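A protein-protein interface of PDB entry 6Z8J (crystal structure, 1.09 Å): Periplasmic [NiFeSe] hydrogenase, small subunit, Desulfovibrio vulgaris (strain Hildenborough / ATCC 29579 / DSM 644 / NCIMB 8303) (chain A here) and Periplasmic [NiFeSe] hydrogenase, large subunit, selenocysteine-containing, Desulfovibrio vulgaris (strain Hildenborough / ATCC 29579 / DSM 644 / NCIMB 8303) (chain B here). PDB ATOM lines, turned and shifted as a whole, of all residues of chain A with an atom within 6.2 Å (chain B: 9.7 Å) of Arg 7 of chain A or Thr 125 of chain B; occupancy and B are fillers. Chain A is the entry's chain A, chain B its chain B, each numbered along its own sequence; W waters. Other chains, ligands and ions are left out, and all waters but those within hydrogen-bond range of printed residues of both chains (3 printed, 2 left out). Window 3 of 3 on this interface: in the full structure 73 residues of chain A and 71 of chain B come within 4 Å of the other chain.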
ATOM      1  N   GLY A   5      11.239 -36.012  22.928  1.00  0.00           N
ATOM      2  CA  GLY A   5      10.978 -34.776  22.206  1.00  0.00           C
ATOM      3  C   GLY A   5      12.236 -33.993  21.872  1.00  0.00           C
ATOM      4  O   GLY A   5      13.193 -33.981  22.653  1.00  0.00           O
ATOM      5  N   GLU A   6      12.238 -33.334  20.713  1.00  0.00           N
ATOM      6  CA  GLU A   6      13.367 -32.536  20.253  1.00  0.00           C
ATOM      7  C   GLU A   6      12.921 -31.088  20.107  1.00  0.00           C
ATOM      8  O   GLU A   6      11.916 -30.804  19.447  1.00  0.00           O
ATOM      9  CB  GLU A   6      13.908 -33.047  18.911  1.00  0.00           C
ATOM     10  CG  GLU A   6      14.209 -34.548  18.864  1.00  0.00           C
ATOM     11  CD  GLU A   6      15.503 -34.932  19.561  1.00  0.00           C
ATOM     12  OE1 GLU A   6      16.439 -34.106  19.587  1.00  0.00           O
ATOM     13  OE2 GLU A   6      15.582 -36.070  20.076  1.00  0.00           O
ATOM     14  N   ARG A   7      13.665 -30.185  20.721  1.00  0.00           N
ATOM     15  CA  ARG A   7      13.290 -28.779  20.734  1.00  0.00           C
ATOM     16  C   ARG A   7      13.452 -28.209  19.333  1.00  0.00           C
ATOM     17  O   ARG A   7      14.577 -28.160  18.827  1.00  0.00           O
ATOM     18  CB  ARG A   7      14.206 -28.017  21.686  1.00  0.00           C
ATOM     19  CG  ARG A   7      14.099 -28.406  23.156  1.00  0.00           C
ATOM     20  CD  ARG A   7      15.449 -28.251  23.848  1.00  0.00           C
ATOM     21  NE  ARG A   7      15.931 -26.871  23.875  1.00  0.00           N
ATOM     22  CZ  ARG A   7      17.212 -26.532  23.885  1.00  0.00           C
ATOM     23  NH1 ARG A   7      18.152 -27.469  23.843  1.00  0.00           N
ATOM     24  NH2 ARG A   7      17.556 -25.259  23.923  1.00  0.00           N
ATOM     25  N   PRO A   8      12.384 -27.757  18.674  1.00  0.00           N
ATOM     26  CA  PRO A   8      12.536 -27.252  17.313  1.00  0.00           C
ATOM     27  C   PRO A   8      13.218 -25.896  17.299  1.00  0.00           C
ATOM     28  O   PRO A   8      13.134 -25.126  18.273  1.00  0.00           O
ATOM     29  CB  PRO A   8      11.085 -27.141  16.819  1.00  0.00           C
ATOM     30  CG  PRO A   8      10.338 -26.834  18.059  1.00  0.00           C
ATOM     31  CD  PRO A   8      10.978 -27.692  19.117  1.00  0.00           C
ATOM     32  N   PRO A   9      13.898 -25.556  16.208  1.00  0.00           N
ATOM     33  CA  PRO A   9      14.512 -24.229  16.098  1.00  0.00           C
ATOM     34  C   PRO A   9      13.469 -23.153  15.878  1.00  0.00           C
ATOM     35  O   PRO A   9      12.515 -23.315  15.113  1.00  0.00           O
ATOM     36  CB  PRO A   9      15.441 -24.367  14.892  1.00  0.00           C
ATOM     37  CG  PRO A   9      14.840 -25.442  14.070  1.00  0.00           C
ATOM     38  CD  PRO A   9      14.144 -26.384  15.012  1.00  0.00           C
ATOM     39  N   VAL A  36      11.103 -22.979  29.134  1.00  0.00           N
ATOM     40  CA  VAL A  36      10.790 -22.832  27.717  1.00  0.00           C
ATOM     41  C   VAL A  36      12.065 -22.876  26.878  1.00  0.00           C
ATOM     42  O   VAL A  36      12.142 -23.585  25.867  1.00  0.00           O
ATOM     43  CB  VAL A  36       9.997 -21.537  27.475  1.00  0.00           C
ATOM     44  CG1 VAL A  36       9.829 -21.299  25.973  1.00  0.00           C
ATOM     45  CG2 VAL A  36       8.640 -21.606  28.167  1.00  0.00           C
ATOM     46  N   LEU A  37      13.089 -22.123  27.291  1.00  0.00           N
ATOM     47  CA  LEU A  37      14.294 -22.002  26.480  1.00  0.00           C
ATOM     48  C   LEU A  37      15.146 -23.256  26.532  1.00  0.00           C
ATOM     49  O   LEU A  37      15.796 -23.597  25.542  1.00  0.00           O
ATOM     50  CB  LEU A  37      15.127 -20.817  26.961  1.00  0.00           C
ATOM     51  CG  LEU A  37      14.518 -19.435  26.783  1.00  0.00           C
ATOM     52  CD1 LEU A  37      15.480 -18.383  27.313  1.00  0.00           C
ATOM     53  CD2 LEU A  37      14.192 -19.159  25.330  1.00  0.00           C
ATOM     54  N   LEU A  38      15.179 -23.941  27.672  1.00  0.00           N
ATOM     55  CA  LEU A  38      16.060 -25.089  27.821  1.00  0.00           C
ATOM     56  C   LEU A  38      15.373 -26.418  27.540  1.00  0.00           C
ATOM     57  O   LEU A  38      16.065 -27.406  27.260  1.00  0.00           O
ATOM     58  CB  LEU A  38      16.662 -25.111  29.235  1.00  0.00           C
ATOM     59  CG  LEU A  38      17.483 -23.859  29.565  1.00  0.00           C
ATOM     60  CD1 LEU A  38      17.926 -23.878  31.010  1.00  0.00           C
ATOM     61  CD2 LEU A  38      18.684 -23.722  28.640  1.00  0.00           C
ATOM     62  N   LYS A  39      14.040 -26.454  27.549  1.00  0.00           N
ATOM     63  CA  LYS A  39      13.316 -27.715  27.412  1.00  0.00           C
ATOM     64  C   LYS A  39      12.288 -27.773  26.297  1.00  0.00           C
ATOM     65  O   LYS A  39      11.900 -28.887  25.913  1.00  0.00           O
ATOM     66  CB  LYS A  39      12.594 -28.062  28.719  1.00  0.00           C
ATOM     67  CG  LYS A  39      13.532 -28.201  29.882  1.00  0.00           C
ATOM     68  CD  LYS A  39      12.784 -28.514  31.148  1.00  0.00           C
ATOM     69  CE  LYS A  39      13.745 -28.815  32.273  1.00  0.00           C
ATOM     70  NZ  LYS A  39      12.981 -29.356  33.430  1.00  0.00           N
ATOM     71  N   VAL A  40      11.789 -26.645  25.801  1.00  0.00           N
ATOM     72  CA  VAL A  40      10.649 -26.625  24.892  1.00  0.00           C
ATOM     73  C   VAL A  40      11.055 -26.212  23.478  1.00  0.00           C
ATOM     74  O   VAL A  40      10.677 -26.862  22.501  1.00  0.00           O
ATOM     75  CB  VAL A  40       9.512 -25.731  25.434  1.00  0.00           C
ATOM     76  CG1 VAL A  40       8.326 -25.800  24.491  1.00  0.00           C
ATOM     77  CG2 VAL A  40       9.104 -26.150  26.844  1.00  0.00           C
ATOM     78  N   ILE A  41      11.814 -25.124  23.347  1.00  0.00           N
ATOM     79  CA  ILE A  41      12.237 -24.631  22.046  1.00  0.00           C
ATOM     80  C   ILE A  41      13.748 -24.463  22.053  1.00  0.00           C
ATOM     81  O   ILE A  41      14.386 -24.450  23.105  1.00  0.00           O
ATOM     82  CB  ILE A  41      11.554 -23.307  21.643  1.00  0.00           C
ATOM     83  CG1 ILE A  41      11.916 -22.158  22.606  1.00  0.00           C
ATOM     84  CG2 ILE A  41      10.044 -23.487  21.553  1.00  0.00           C
ATOM     85  CD1 ILE A  41      11.447 -20.793  22.124  1.00  0.00           C
ATOM     86  N   SER A  42      14.312 -24.324  20.855  1.00  0.00           N
ATOM     87  CA  SER A  42      15.693 -23.898  20.688  1.00  0.00           C
ATOM     88  C   SER A  42      15.653 -22.529  20.022  1.00  0.00           C
ATOM     89  O   SER A  42      15.451 -22.420  18.811  1.00  0.00           O
ATOM     90  CB  SER A  42      16.480 -24.892  19.847  1.00  0.00           C
ATOM     91  OG  SER A  42      17.830 -24.480  19.824  1.00  0.00           O
ATOM     92  N   LEU A  43      15.821 -21.489  20.827  1.00  0.00           N
ATOM     93  CA  LEU A  43      15.716 -20.107  20.374  1.00  0.00           C
ATOM     94  C   LEU A  43      17.052 -19.719  19.752  1.00  0.00           C
ATOM     95  O   LEU A  43      17.971 -19.275  20.432  1.00  0.00           O
ATOM     96  CB  LEU A  43      15.325 -19.193  21.528  1.00  0.00           C
ATOM     97  CG  LEU A  43      15.051 -17.742  21.144  1.00  0.00           C
ATOM     98  CD1 LEU A  43      13.905 -17.588  20.155  1.00  0.00           C
ATOM     99  CD2 LEU A  43      14.823 -16.922  22.383  1.00  0.00           C
ATOM    100  N   GLU A  44      17.148 -19.895  18.432  1.00  0.00           N
ATOM    101  CA  GLU A  44      18.418 -19.776  17.722  1.00  0.00           C
ATOM    102  C   GLU A  44      18.768 -18.341  17.372  1.00  0.00           C
ATOM    103  O   GLU A  44      19.951 -18.031  17.258  1.00  0.00           O
ATOM    104  CB  GLU A  44      18.394 -20.623  16.450  1.00  0.00           C
ATOM    105  CG  GLU A  44      18.285 -22.117  16.739  1.00  0.00           C
ATOM    106  CD  GLU A  44      19.565 -22.720  17.349  1.00  0.00           C
ATOM    107  OE1 GLU A  44      20.620 -22.059  17.259  1.00  0.00           O
ATOM    108  OE2 GLU A  44      19.503 -23.850  17.920  1.00  0.00           O
ATOM    109  N   GLN B 117      26.108 -11.766  29.674  1.00  0.00           N
ATOM    110  CA  GLN B 117      26.764 -12.615  28.689  1.00  0.00           C
ATOM    111  C   GLN B 117      27.988 -11.955  28.064  1.00  0.00           C
ATOM    112  O   GLN B 117      28.782 -12.661  27.442  1.00  0.00           O
ATOM    113  CB  GLN B 117      25.778 -13.050  27.609  1.00  0.00           C
ATOM    114  CG  GLN B 117      24.856 -14.169  28.058  1.00  0.00           C
ATOM    115  CD  GLN B 117      24.200 -14.856  26.883  1.00  0.00           C
ATOM    116  OE1 GLN B 117      24.819 -15.695  26.202  1.00  0.00           O
ATOM    117  NE2 GLN B 117      22.961 -14.488  26.614  1.00  0.00           N
ATOM    118  N   GLN B 121      30.029 -17.011  30.196  1.00  0.00           N
ATOM    119  CA  GLN B 121      29.662 -18.016  29.204  1.00  0.00           C
ATOM    120  C   GLN B 121      28.421 -18.757  29.680  1.00  0.00           C
ATOM    121  O   GLN B 121      28.444 -19.407  30.731  1.00  0.00           O
ATOM    122  CB  GLN B 121      30.806 -19.006  29.010  1.00  0.00           C
ATOM    123  CG  GLN B 121      30.467 -20.224  28.117  1.00  0.00           C
ATOM    124  CD  GLN B 121      30.096 -19.825  26.681  1.00  0.00           C
ATOM    125  OE1 GLN B 121      30.921 -19.290  25.947  1.00  0.00           O
ATOM    126  NE2 GLN B 121      28.846 -20.084  26.287  1.00  0.00           N
ATOM    127  N   GLY B 122      27.347 -18.675  28.903  1.00  0.00           N
ATOM    128  CA  GLY B 122      26.139 -19.395  29.220  1.00  0.00           C
ATOM    129  C   GLY B 122      26.212 -20.862  28.839  1.00  0.00           C
ATOM    130  O   GLY B 122      27.208 -21.358  28.304  1.00  0.00           O
ATOM    131  N   PRO B 123      25.130 -21.582  29.138  1.00  0.00           N
ATOM    132  CA  PRO B 123      25.056 -23.008  28.813  1.00  0.00           C
ATOM    133  C   PRO B 123      25.247 -23.264  27.327  1.00  0.00           C
ATOM    134  O   PRO B 123      24.989 -22.404  26.485  1.00  0.00           O
ATOM    135  CB  PRO B 123      23.637 -23.395  29.254  1.00  0.00           C
ATOM    136  CG  PRO B 123      23.216 -22.352  30.199  1.00  0.00           C
ATOM    137  CD  PRO B 123      23.933 -21.100  29.845  1.00  0.00           C
ATOM    138  N   ASP B 124      25.680 -24.484  27.002  1.00  0.00           N
ATOM    139  CA  ASP B 124      26.052 -24.822  25.630  1.00  0.00           C
ATOM    140  C   ASP B 124      24.821 -25.167  24.785  1.00  0.00           C
ATOM    141  O   ASP B 124      24.684 -26.265  24.241  1.00  0.00           O
ATOM    142  CB  ASP B 124      27.070 -25.949  25.617  1.00  0.00           C
ATOM    143  CG  ASP B 124      27.606 -26.222  24.232  1.00  0.00           C
ATOM    144  OD1 ASP B 124      27.609 -25.301  23.393  1.00  0.00           O
ATOM    145  OD2 ASP B 124      28.028 -27.362  23.973  1.00  0.00           O
ATOM    146  N   THR B 125      23.930 -24.185  24.668  1.00  0.00           N
ATOM    147  CA  THR B 125      22.744 -24.328  23.841  1.00  0.00           C
ATOM    148  C   THR B 125      22.246 -22.932  23.484  1.00  0.00           C
ATOM    149  O   THR B 125      22.544 -21.954  24.174  1.00  0.00           O
ATOM    150  CB  THR B 125      21.677 -25.159  24.553  1.00  0.00           C
ATOM    151  OG1 THR B 125      20.741 -25.636  23.580  1.00  0.00           O
ATOM    152  CG2 THR B 125      20.978 -24.349  25.648  1.00  0.00           C
ATOM    153  N   ALA B 126      21.511 -22.840  22.374  1.00  0.00           N
ATOM    154  CA  ALA B 126      20.940 -21.558  21.989  1.00  0.00           C
ATOM    155  C   ALA B 126      19.999 -21.070  23.090  1.00  0.00           C
ATOM    156  O   ALA B 126      19.304 -21.882  23.705  1.00  0.00           O
ATOM    157  CB  ALA B 126      20.162 -21.706  20.679  1.00  0.00           C
ATOM    158  N   PRO B 127      19.926 -19.755  23.344  1.00  0.00           N
ATOM    159  CA  PRO B 127      20.539 -18.648  22.603  1.00  0.00           C
ATOM    160  C   PRO B 127      21.919 -18.215  23.113  1.00  0.00           C
ATOM    161  O   PRO B 127      22.343 -17.113  22.819  1.00  0.00           O
ATOM    162  CB  PRO B 127      19.522 -17.530  22.818  1.00  0.00           C
ATOM    163  CG  PRO B 127      19.065 -17.770  24.236  1.00  0.00           C
ATOM    164  CD  PRO B 127      18.998 -19.261  24.380  1.00  0.00           C
ATOM    165  N   PHE B 128      22.604 -19.074  23.859  1.00  0.00           N
ATOM    166  CA  PHE B 128      23.864 -18.718  24.501  1.00  0.00           C
ATOM    167  C   PHE B 128      25.070 -19.066  23.644  1.00  0.00           C
ATOM    168  O   PHE B 128      26.189 -18.655  23.978  1.00  0.00           O
ATOM    169  CB  PHE B 128      23.987 -19.440  25.851  1.00  0.00           C
ATOM    170  CG  PHE B 128      22.828 -19.197  26.763  1.00  0.00           C
ATOM    171  CD1 PHE B 128      22.773 -18.052  27.522  1.00  0.00           C
ATOM    172  CD2 PHE B 128      21.783 -20.117  26.864  1.00  0.00           C
ATOM    173  CE1 PHE B 128      21.702 -17.828  28.363  1.00  0.00           C
ATOM    174  CE2 PHE B 128      20.721 -19.892  27.689  1.00  0.00           C
ATOM    175  CZ  PHE B 128      20.678 -18.751  28.444  1.00  0.00           C
ATOM    176  N   VAL B 129      24.844 -19.818  22.571  1.00  0.00           N
ATOM    177  CA  VAL B 129      25.840 -20.174  21.563  1.00  0.00           C
ATOM    178  C   VAL B 129      25.146 -20.175  20.211  1.00  0.00           C
ATOM    179  O   VAL B 129      23.919 -20.304  20.129  1.00  0.00           O
ATOM    180  CB  VAL B 129      26.465 -21.557  21.834  1.00  0.00           C
ATOM    181  CG1 VAL B 129      27.192 -21.556  23.156  1.00  0.00           C
ATOM    182  CG2 VAL B 129      25.416 -22.649  21.833  1.00  0.00           C
ATOM    183  N   PRO B 130      25.910 -20.032  19.125  1.00  0.00           N
ATOM    184  CA  PRO B 130      27.333 -19.701  19.077  1.00  0.00           C
ATOM    185  C   PRO B 130      27.615 -18.237  19.397  1.00  0.00           C
ATOM    186  O   PRO B 130      26.700 -17.424  19.499  1.00  0.00           O
ATOM    187  CB  PRO B 130      27.706 -19.998  17.625  1.00  0.00           C
ATOM    188  CG  PRO B 130      26.441 -19.718  16.857  1.00  0.00           C
ATOM    189  CD  PRO B 130      25.307 -20.092  17.784  1.00  0.00           C
ATOM    190  N   ARG B 131      28.892 -17.911  19.552  1.00  0.00           N
ATOM    191  CA  ARG B 131      29.296 -16.547  19.862  1.00  0.00           C
ATOM    192  C   ARG B 131      30.722 -16.357  19.355  1.00  0.00           C
ATOM    193  O   ARG B 131      31.282 -17.237  18.699  1.00  0.00           O
ATOM    194  CB  ARG B 131      29.107 -16.230  21.354  1.00  0.00           C
ATOM    195  CG  ARG B 131      29.890 -17.115  22.311  1.00  0.00           C
ATOM    196  CD  ARG B 131      29.560 -16.743  23.747  1.00  0.00           C
ATOM    197  NE  ARG B 131      29.975 -15.368  23.998  1.00  0.00           N
ATOM    198  CZ  ARG B 131      29.681 -14.652  25.078  1.00  0.00           C
ATOM    199  NH1 ARG B 131      28.953 -15.167  26.046  1.00  0.00           N
ATOM    200  NH2 ARG B 131      30.131 -13.410  25.181  1.00  0.00           N
ATOM    201  N   TYR B 151      21.911 -15.490  36.707  1.00  0.00           N
ATOM    202  CA  TYR B 151      21.106 -15.191  35.531  1.00  0.00           C
ATOM    203  C   TYR B 151      19.780 -15.931  35.635  1.00  0.00           C
ATOM    204  O   TYR B 151      18.702 -15.357  35.443  1.00  0.00           O
ATOM    205  CB  TYR B 151      21.893 -15.645  34.293  1.00  0.00           C
ATOM    206  CG  TYR B 151      21.196 -15.525  32.947  1.00  0.00           C
ATOM    207  CD1 TYR B 151      20.148 -16.365  32.588  1.00  0.00           C
ATOM    208  CD2 TYR B 151      21.631 -14.594  32.005  1.00  0.00           C
ATOM    209  CE1 TYR B 151      19.541 -16.265  31.334  1.00  0.00           C
ATOM    210  CE2 TYR B 151      21.041 -14.507  30.753  1.00  0.00           C
ATOM    211  CZ  TYR B 151      19.987 -15.334  30.428  1.00  0.00           C
ATOM    212  OH  TYR B 151      19.387 -15.233  29.196  1.00  0.00           O
ATOM    213  N   ILE B 152      19.848 -17.220  35.954  1.00  0.00           N
ATOM    214  CA  ILE B 152      18.642 -18.036  36.022  1.00  0.00           C
ATOM    215  C   ILE B 152      17.743 -17.580  37.166  1.00  0.00           C
ATOM    216  O   ILE B 152      16.523 -17.446  37.002  1.00  0.00           O
ATOM    217  CB  ILE B 152      19.016 -19.527  36.133  1.00  0.00           C
ATOM    218  CG1 ILE B 152      19.736 -20.018  34.858  1.00  0.00           C
ATOM    219  CG2 ILE B 152      17.781 -20.377  36.437  1.00  0.00           C
ATOM    220  CD1 ILE B 152      18.865 -20.083  33.605  1.00  0.00           C
HETATM  221  O   HOH W   1      22.878 -22.711  18.847  1.00  0.00           O
HETATM  222  O   HOH W   2      21.940 -18.289  19.391  1.00  0.00           O
HETATM  223  O   HOH W   3      21.571 -24.604  19.874  1.00  0.00           O
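The guanidinium group (NH1) of Arg 7 of chain A is in hydrogen-bond range of the side-chain hydroxyl (OG1) of Thr 125 of chain B (3.2 Å).
The guanidinium group of Arg 7 of chain A lies within hydrogen-bond range of the backbone carbonyl oxygen of Leu 37 of chain A (2.9 Å).
The guanidinium group (NE) of Arg 7 of chain A lies within hydrogen-bond range of the backbone carbonyl oxygen (O) of Leu 38 of chain A, at 3.4 Å.
The guanidinium group (NE) of Arg 7 of chain A lies within hydrogen-bond range of the backbone carbonyl oxygen (O) of Ile 41 of chain A.
The backbone carbonyl oxygen (O) of Pro 8 of chain A is in hydrogen-bond range of the backbone NH (N) of Ser 42 of chain A.
The side-chain hydroxyl (OG) of Ser 42 of chain A is in hydrogen-bond range of the side-chain carboxylate (OE2) of Glu 44 of chain A, 2.6 Å away.
Arg 7 of chain A touches Ala 126 of chain B (NH2 to O, 3.8 Å).
Leu 38 of chain A touches Thr 125 of chain B (CD2 to CG2, 3.8 Å).
OG of Ser 42 of chain A touches CB of Ala 126 of chain B, at 3.7 Å.
Leu 43 of chain A touches Ala 126 of chain B (O to CB, 3.3 Å).
Leu 43 of chain A touches Pro 127 of chain B (O to CB, 3.3 Å).
Ala 126 of chain B touches Glu 44 of chain A.
Arg 7 of chain A touches two residues of chain B.
Thr 125 of chain B touches just these residues of chain A: Arg 7 (3.2 Å) and Leu 38 (3.8 Å).
No residue of chain B comes within 4 Å of Pro 8 of chain A.
Printed residues of chain A within 4 Å of Ala 126 of chain B: Arg 7, Ser 42, Leu 43 and Glu 44.
Of the printed residues of chain B, Glu 44 of chain A touches Ala 126 (3.5 Å).
Val 129 of chain B touches none of the printed residues of chain A.
The nearest residue of chain B that does not touch Arg 7 of chain A is Pro 127 of chain B (6.0 Å).
The nearest residue of chain A that does not touch Thr 125 of chain B is Ser 42 of chain A (4.9 Å).
Of the 14 printed residues of chain A, 5 touch a printed residue of chain B.
Hydrophobic or aromatic side chains of chain A that line the printed part of chain B: Leu 38.
Of the 14 printed residues of chain B, 3 touch a printed residue of chain A.
Printed residues of chain B that touch a printed residue of chain A: Thr 125, Ala 126 and Pro 127.
Among the printed residues, no Asp or Glu carboxylate lies within 4 Å of a Lys or Arg side-chain nitrogen of the other chain.
Water W1 bridges the side-chain carboxylate of Glu 44 of chain A and the backbone carbonyl oxygen of Val 129 of chain B.
Water W2 bridges the backbone carbonyl oxygen (O) of Val 129 of chain B (2.9 Å) and the backbone carbonyl oxygen (O) of Glu 44 of chain A (2.9 Å).
Water W3 bridges the side-chain carboxylate of Glu 44 of chain A (2.9 Å) and the backbone NH of Ala 126 of chain B (3.1 Å).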
